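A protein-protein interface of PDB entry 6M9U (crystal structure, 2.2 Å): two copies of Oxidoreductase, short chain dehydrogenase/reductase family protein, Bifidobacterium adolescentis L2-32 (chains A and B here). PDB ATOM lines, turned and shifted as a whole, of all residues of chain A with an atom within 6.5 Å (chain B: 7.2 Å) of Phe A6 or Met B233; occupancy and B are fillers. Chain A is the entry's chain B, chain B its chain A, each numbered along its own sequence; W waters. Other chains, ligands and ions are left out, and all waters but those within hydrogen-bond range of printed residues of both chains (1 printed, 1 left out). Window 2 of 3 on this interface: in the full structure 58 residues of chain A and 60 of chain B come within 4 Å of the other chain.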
ATOM      1  N   VAL A   2     -18.862   6.146  15.292  1.00  0.00           N
ATOM      2  CA  VAL A   2     -17.529   6.179  14.689  1.00  0.00           C
ATOM      3  C   VAL A   2     -16.881   7.523  15.014  1.00  0.00           C
ATOM      4  O   VAL A   2     -15.836   7.577  15.674  1.00  0.00           O
ATOM      5  CB  VAL A   2     -17.603   5.920  13.170  1.00  0.00           C
ATOM      6  CG1 VAL A   2     -16.330   6.375  12.458  1.00  0.00           C
ATOM      7  CG2 VAL A   2     -17.858   4.429  12.893  1.00  0.00           C
ATOM      8  N   GLU A   3     -17.494   8.615  14.554  1.00  0.00           N
ATOM      9  CA  GLU A   3     -17.049   9.961  14.891  1.00  0.00           C
ATOM     10  C   GLU A   3     -17.641  10.440  16.214  1.00  0.00           C
ATOM     11  O   GLU A   3     -16.967  11.138  16.973  1.00  0.00           O
ATOM     12  CB  GLU A   3     -17.430  10.948  13.780  1.00  0.00           C
ATOM     13  CG  GLU A   3     -16.281  11.399  12.877  1.00  0.00           C
ATOM     14  CD  GLU A   3     -16.235  10.672  11.533  1.00  0.00           C
ATOM     15  OE1 GLU A   3     -16.717   9.519  11.437  1.00  0.00           O
ATOM     16  OE2 GLU A   3     -15.711  11.260  10.564  1.00  0.00           O
ATOM     17  N   GLN A   4     -18.896  10.080  16.497  1.00  0.00           N
ATOM     18  CA  GLN A   4     -19.570  10.453  17.744  1.00  0.00           C
ATOM     19  C   GLN A   4     -19.090   9.544  18.880  1.00  0.00           C
ATOM     20  O   GLN A   4     -19.818   8.721  19.436  1.00  0.00           O
ATOM     21  CB  GLN A   4     -21.084  10.375  17.578  1.00  0.00           C
ATOM     22  CG  GLN A   4     -21.575   9.005  17.121  1.00  0.00           C
ATOM     23  CD  GLN A   4     -23.070   8.838  17.270  1.00  0.00           C
ATOM     24  OE1 GLN A   4     -23.814   9.818  17.299  1.00  0.00           O
ATOM     25  NE2 GLN A   4     -23.516   7.594  17.376  1.00  0.00           N
ATOM     26  N   ILE A   5     -17.815   9.696  19.198  1.00  0.00           N
ATOM     27  CA  ILE A   5     -17.154   9.080  20.344  1.00  0.00           C
ATOM     28  C   ILE A   5     -16.119  10.145  20.710  1.00  0.00           C
ATOM     29  O   ILE A   5     -16.059  10.637  21.840  1.00  0.00           O
ATOM     30  CB  ILE A   5     -16.506   7.725  20.021  1.00  0.00           C
ATOM     31  CG1 ILE A   5     -17.569   6.617  19.936  1.00  0.00           C
ATOM     32  CG2 ILE A   5     -15.425   7.391  21.063  1.00  0.00           C
ATOM     33  CD1 ILE A   5     -17.473   5.532  21.020  1.00  0.00           C
ATOM     34  N   PHE A   6     -15.305  10.515  19.712  1.00  0.00           N
ATOM     35  CA  PHE A   6     -14.472  11.705  19.803  1.00  0.00           C
ATOM     36  C   PHE A   6     -15.295  12.931  20.187  1.00  0.00           C
ATOM     37  O   PHE A   6     -14.827  13.783  20.952  1.00  0.00           O
ATOM     38  CB  PHE A   6     -13.748  11.923  18.471  1.00  0.00           C
ATOM     39  CG  PHE A   6     -12.678  10.898  18.191  1.00  0.00           C
ATOM     40  CD1 PHE A   6     -11.846  10.457  19.205  1.00  0.00           C
ATOM     41  CD2 PHE A   6     -12.504  10.371  16.922  1.00  0.00           C
ATOM     42  CE1 PHE A   6     -10.867   9.519  18.965  1.00  0.00           C
ATOM     43  CE2 PHE A   6     -11.518   9.430  16.677  1.00  0.00           C
ATOM     44  CZ  PHE A   6     -10.701   9.006  17.705  1.00  0.00           C
ATOM     45  N   ASP A   7     -16.526  13.039  19.680  1.00  0.00           N
ATOM     46  CA  ASP A   7     -17.363  14.181  20.023  1.00  0.00           C
ATOM     47  C   ASP A   7     -17.919  14.056  21.439  1.00  0.00           C
ATOM     48  O   ASP A   7     -18.194  15.076  22.086  1.00  0.00           O
ATOM     49  CB  ASP A   7     -18.494  14.334  18.995  1.00  0.00           C
ATOM     50  CG  ASP A   7     -17.977  14.702  17.587  1.00  0.00           C
ATOM     51  OD1 ASP A   7     -16.789  15.072  17.452  1.00  0.00           O
ATOM     52  OD2 ASP A   7     -18.760  14.612  16.611  1.00  0.00           O
ATOM     53  N   GLU A   8     -18.054  12.831  21.955  1.00  0.00           N
ATOM     54  CA  GLU A   8     -18.575  12.653  23.310  1.00  0.00           C
ATOM     55  C   GLU A   8     -17.481  12.837  24.367  1.00  0.00           C
ATOM     56  O   GLU A   8     -17.719  13.430  25.433  1.00  0.00           O
ATOM     57  CB  GLU A   8     -19.237  11.271  23.452  1.00  0.00           C
ATOM     58  CG  GLU A   8     -20.615  11.138  22.757  1.00  0.00           C
ATOM     59  CD  GLU A   8     -21.357   9.836  23.089  1.00  0.00           C
ATOM     60  OE1 GLU A   8     -20.995   9.161  24.087  1.00  0.00           O
ATOM     61  OE2 GLU A   8     -22.309   9.493  22.346  1.00  0.00           O
ATOM     62  N   ARG A   9     -16.276  12.344  24.103  1.00  0.00           N
ATOM     63  CA  ARG A   9     -15.206  12.454  25.081  1.00  0.00           C
ATOM     64  C   ARG A   9     -14.338  13.692  24.879  1.00  0.00           C
ATOM     65  O   ARG A   9     -13.493  13.975  25.732  1.00  0.00           O
ATOM     66  CB  ARG A   9     -14.340  11.184  25.068  1.00  0.00           C
ATOM     67  CG  ARG A   9     -13.544  10.933  23.811  1.00  0.00           C
ATOM     68  CD  ARG A   9     -12.566   9.734  23.930  1.00  0.00           C
ATOM     69  NE  ARG A   9     -13.213   8.432  24.117  1.00  0.00           N
ATOM     70  CZ  ARG A   9     -12.652   7.258  23.820  1.00  0.00           C
ATOM     71  NH1 ARG A   9     -11.432   7.203  23.299  1.00  0.00           N
ATOM     72  NH2 ARG A   9     -13.319   6.134  24.038  1.00  0.00           N
ATOM     73  N   TYR A  10     -14.546  14.458  23.805  1.00  0.00           N
ATOM     74  CA  TYR A  10     -13.759  15.657  23.538  1.00  0.00           C
ATOM     75  C   TYR A  10     -14.656  16.770  23.024  1.00  0.00           C
ATOM     76  O   TYR A  10     -14.547  17.206  21.872  1.00  0.00           O
ATOM     77  CB  TYR A  10     -12.650  15.378  22.521  1.00  0.00           C
ATOM     78  CG  TYR A  10     -11.575  14.403  22.936  1.00  0.00           C
ATOM     79  CD1 TYR A  10     -10.926  14.518  24.156  1.00  0.00           C
ATOM     80  CD2 TYR A  10     -11.203  13.376  22.087  1.00  0.00           C
ATOM     81  CE1 TYR A  10      -9.945  13.645  24.511  1.00  0.00           C
ATOM     82  CE2 TYR A  10     -10.231  12.494  22.435  1.00  0.00           C
ATOM     83  CZ  TYR A  10      -9.594  12.640  23.650  1.00  0.00           C
ATOM     84  OH  TYR A  10      -8.603  11.767  24.006  1.00  0.00           O
ATOM     85  N   PRO A  11     -15.515  17.306  23.869  1.00  0.00           N
ATOM     86  CA  PRO A  11     -16.264  18.493  23.463  1.00  0.00           C
ATOM     87  C   PRO A  11     -15.307  19.586  23.010  1.00  0.00           C
ATOM     88  O   PRO A  11     -14.210  19.758  23.554  1.00  0.00           O
ATOM     89  CB  PRO A  11     -17.023  18.893  24.730  1.00  0.00           C
ATOM     90  CG  PRO A  11     -16.851  17.774  25.670  1.00  0.00           C
ATOM     91  CD  PRO A  11     -15.614  17.043  25.306  1.00  0.00           C
ATOM     92  N   TRP B 223      -7.693  18.734  21.473  1.00  0.00           N
ATOM     93  CA  TRP B 223      -8.640  18.289  20.454  1.00  0.00           C
ATOM     94  C   TRP B 223      -9.424  19.450  19.865  1.00  0.00           C
ATOM     95  O   TRP B 223     -10.153  20.119  20.608  1.00  0.00           O
ATOM     96  CB  TRP B 223      -9.604  17.291  21.079  1.00  0.00           C
ATOM     97  CG  TRP B 223     -10.551  16.720  20.132  1.00  0.00           C
ATOM     98  CD1 TRP B 223     -11.826  17.133  19.888  1.00  0.00           C
ATOM     99  CD2 TRP B 223     -10.314  15.604  19.281  1.00  0.00           C
ATOM    100  NE1 TRP B 223     -12.396  16.338  18.934  1.00  0.00           N
ATOM    101  CE2 TRP B 223     -11.489  15.390  18.540  1.00  0.00           C
ATOM    102  CE3 TRP B 223      -9.216  14.764  19.071  1.00  0.00           C
ATOM    103  CZ2 TRP B 223     -11.606  14.367  17.609  1.00  0.00           C
ATOM    104  CZ3 TRP B 223      -9.338  13.736  18.143  1.00  0.00           C
ATOM    105  CH2 TRP B 223     -10.532  13.542  17.433  1.00  0.00           C
ATOM    106  N   GLY B 225     -11.215  18.632  16.482  1.00  0.00           N
ATOM    107  CA  GLY B 225     -11.906  18.021  15.356  1.00  0.00           C
ATOM    108  C   GLY B 225     -11.042  17.606  14.184  1.00  0.00           C
ATOM    109  O   GLY B 225     -11.148  16.478  13.697  1.00  0.00           O
ATOM    110  N   ASP B 232      -8.803   8.957  12.999  1.00  0.00           N
ATOM    111  CA  ASP B 232      -8.782   7.508  13.161  1.00  0.00           C
ATOM    112  C   ASP B 232      -8.426   7.057  14.597  1.00  0.00           C
ATOM    113  O   ASP B 232      -7.409   7.498  15.122  1.00  0.00           O
ATOM    114  CB  ASP B 232      -7.782   6.889  12.175  1.00  0.00           C
ATOM    115  CG  ASP B 232      -7.938   5.393  12.056  1.00  0.00           C
ATOM    116  OD1 ASP B 232      -8.984   4.871  12.493  1.00  0.00           O
ATOM    117  OD2 ASP B 232      -7.020   4.734  11.526  1.00  0.00           O
ATOM    118  N   MET B 233      -9.260   6.159  15.153  1.00  0.00           N
ATOM    119  CA  MET B 233      -9.064   5.732  16.540  1.00  0.00           C
ATOM    120  C   MET B 233      -7.694   5.133  16.831  1.00  0.00           C
ATOM    121  O   MET B 233      -7.221   5.308  17.974  1.00  0.00           O
ATOM    122  CB  MET B 233     -10.172   4.706  16.895  1.00  0.00           C
ATOM    123  CG  MET B 233     -10.422   4.465  18.396  1.00  0.00           C
ATOM    124  SD  MET B 233      -9.087   3.595  19.261  1.00  0.00           S
ATOM    125  CE  MET B 233      -9.864   3.095  20.798  1.00  0.00           C
ATOM    126  N   PRO B 234      -7.048   4.402  15.941  1.00  0.00           N
ATOM    127  CA  PRO B 234      -5.647   4.037  16.198  1.00  0.00           C
ATOM    128  C   PRO B 234      -4.638   5.156  15.973  1.00  0.00           C
ATOM    129  O   PRO B 234      -3.625   5.199  16.675  1.00  0.00           O
ATOM    130  CB  PRO B 234      -5.399   2.865  15.229  1.00  0.00           C
ATOM    131  CG  PRO B 234      -6.539   2.892  14.259  1.00  0.00           C
ATOM    132  CD  PRO B 234      -7.702   3.451  15.025  1.00  0.00           C
ATOM    133  N   GLY B 235      -4.871   6.050  15.011  1.00  0.00           N
ATOM    134  CA  GLY B 235      -4.063   7.256  14.931  1.00  0.00           C
ATOM    135  C   GLY B 235      -4.242   8.172  16.130  1.00  0.00           C
ATOM    136  O   GLY B 235      -3.429   9.077  16.346  1.00  0.00           O
ATOM    137  N   HIS B 236      -5.314   7.967  16.896  1.00  0.00           N
ATOM    138  CA  HIS B 236      -5.555   8.565  18.208  1.00  0.00           C
ATOM    139  C   HIS B 236      -4.482   8.106  19.179  1.00  0.00           C
ATOM    140  O   HIS B 236      -3.537   8.855  19.456  1.00  0.00           O
ATOM    141  CB  HIS B 236      -6.963   8.153  18.644  1.00  0.00           C
ATOM    142  CG  HIS B 236      -7.410   8.699  19.964  1.00  0.00           C
ATOM    143  ND1 HIS B 236      -7.430   7.936  21.112  1.00  0.00           N
ATOM    144  CD2 HIS B 236      -7.959   9.891  20.299  1.00  0.00           C
ATOM    145  CE1 HIS B 236      -7.927   8.648  22.108  1.00  0.00           C
ATOM    146  NE2 HIS B 236      -8.261   9.837  21.639  1.00  0.00           N
ATOM    147  N   ASP B 237      -4.587   6.860  19.657  1.00  0.00           N
ATOM    148  CA  ASP B 237      -3.616   6.299  20.589  1.00  0.00           C
ATOM    149  C   ASP B 237      -2.194   6.360  20.045  1.00  0.00           C
ATOM    150  O   ASP B 237      -1.230   6.106  20.770  1.00  0.00           O
ATOM    151  CB  ASP B 237      -3.965   4.838  20.909  1.00  0.00           C
ATOM    152  CG  ASP B 237      -5.389   4.669  21.383  1.00  0.00           C
ATOM    153  OD1 ASP B 237      -5.691   5.049  22.537  1.00  0.00           O
ATOM    154  OD2 ASP B 237      -6.212   4.170  20.587  1.00  0.00           O
ATOM    155  N   ALA B 238      -2.066   6.684  18.763  1.00  0.00           N
ATOM    156  CA  ALA B 238      -0.757   6.833  18.146  1.00  0.00           C
ATOM    157  C   ALA B 238       0.064   7.907  18.847  1.00  0.00           C
ATOM    158  O   ALA B 238       1.125   7.619  19.400  1.00  0.00           O
ATOM    159  CB  ALA B 238      -0.928   7.166  16.661  1.00  0.00           C
ATOM    160  N   LEU B 240      -0.998   9.739  21.407  1.00  0.00           N
ATOM    161  CA  LEU B 240      -1.185   9.703  22.842  1.00  0.00           C
ATOM    162  C   LEU B 240      -0.216   8.752  23.534  1.00  0.00           C
ATOM    163  O   LEU B 240      -0.091   8.842  24.747  1.00  0.00           O
ATOM    164  CB  LEU B 240      -2.624   9.338  23.157  1.00  0.00           C
ATOM    165  CG  LEU B 240      -3.589  10.361  22.565  1.00  0.00           C
ATOM    166  CD1 LEU B 240      -4.975  10.004  22.929  1.00  0.00           C
ATOM    167  CD2 LEU B 240      -3.308  11.784  23.013  1.00  0.00           C
ATOM    168  N   PHE B 248      -6.051  13.498  24.706  1.00  0.00           N
ATOM    169  CA  PHE B 248      -5.991  14.895  24.328  1.00  0.00           C
ATOM    170  C   PHE B 248      -6.581  15.759  25.422  1.00  0.00           C
ATOM    171  O   PHE B 248      -7.530  15.375  26.087  1.00  0.00           O
ATOM    172  CB  PHE B 248      -6.819  15.183  23.053  1.00  0.00           C
ATOM    173  CG  PHE B 248      -6.228  14.615  21.796  1.00  0.00           C
ATOM    174  CD1 PHE B 248      -6.509  13.318  21.402  1.00  0.00           C
ATOM    175  CD2 PHE B 248      -5.420  15.382  21.003  1.00  0.00           C
ATOM    176  CE1 PHE B 248      -5.961  12.797  20.251  1.00  0.00           C
ATOM    177  CE2 PHE B 248      -4.877  14.869  19.850  1.00  0.00           C
ATOM    178  CZ  PHE B 248      -5.130  13.577  19.479  1.00  0.00           C
HETATM  179  O   HOH W   1     -11.829  20.537  22.894  1.00  0.00           O
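The side-chain hydroxyl (OH) of Tyr A10 is in hydrogen-bond range of a ring nitrogen (NE2) of His B236. The backbone NH of Phe B248 lies within hydrogen-bond range of the side-chain hydroxyl of Tyr A10, 3.2 Å away.
Trp B223 touches Phe A6 (CZ2 to CB, 3.4 Å). CZ of Phe A6 touches CA of Met B233, 3.8 Å away. Phe A6 touches His B236. CE1 of His B236 touches NH1 of Arg A9 (3.97 Å). Tyr A10 touches Trp B223.
Of the printed residues of chain B, Tyr A10 touches Trp B223 (3.3 Å), His B236 (3.1 Å) and Phe B248 (3.2 Å). Met B233 touches just one residue of chain A: Phe A6. Of the printed residues of chain A, His B236 touches Phe A6 (3.2 Å), Arg A9 (3.97 Å) and Tyr A10 (3.1 Å). The nearest residue of chain A that does not touch Met B233 is Arg A9 (5.1 Å). The nearest printed residue of chain A that does not touch Phe B248 is Phe A6 (6.0 Å).
Hydrophobic or aromatic side chains of chain B within 4 Å of the printed part of chain A: Trp B223, His B236 and Phe B248. Of the 10 printed residues of chain A, 3 touch a printed residue of chain B. Hydrophobic or aromatic side chains of chain A that line the printed part of chain B: Phe A6 and Tyr A10. Among the printed residues, 7 pairs touch across the chains. Among the printed residues, no Asp or Glu carboxylate lies within 4 Å of a Lys or Arg side-chain nitrogen of the other chain.
No position is printed for both chains. Of the 7 pairs that touch across the chains among the printed residues, none has its exchanged pair printed and touching as well.
Water W1 lies within hydrogen-bond range of O of Pro A11 (2.6 Å) and O of Trp B223 (2.9 Å).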
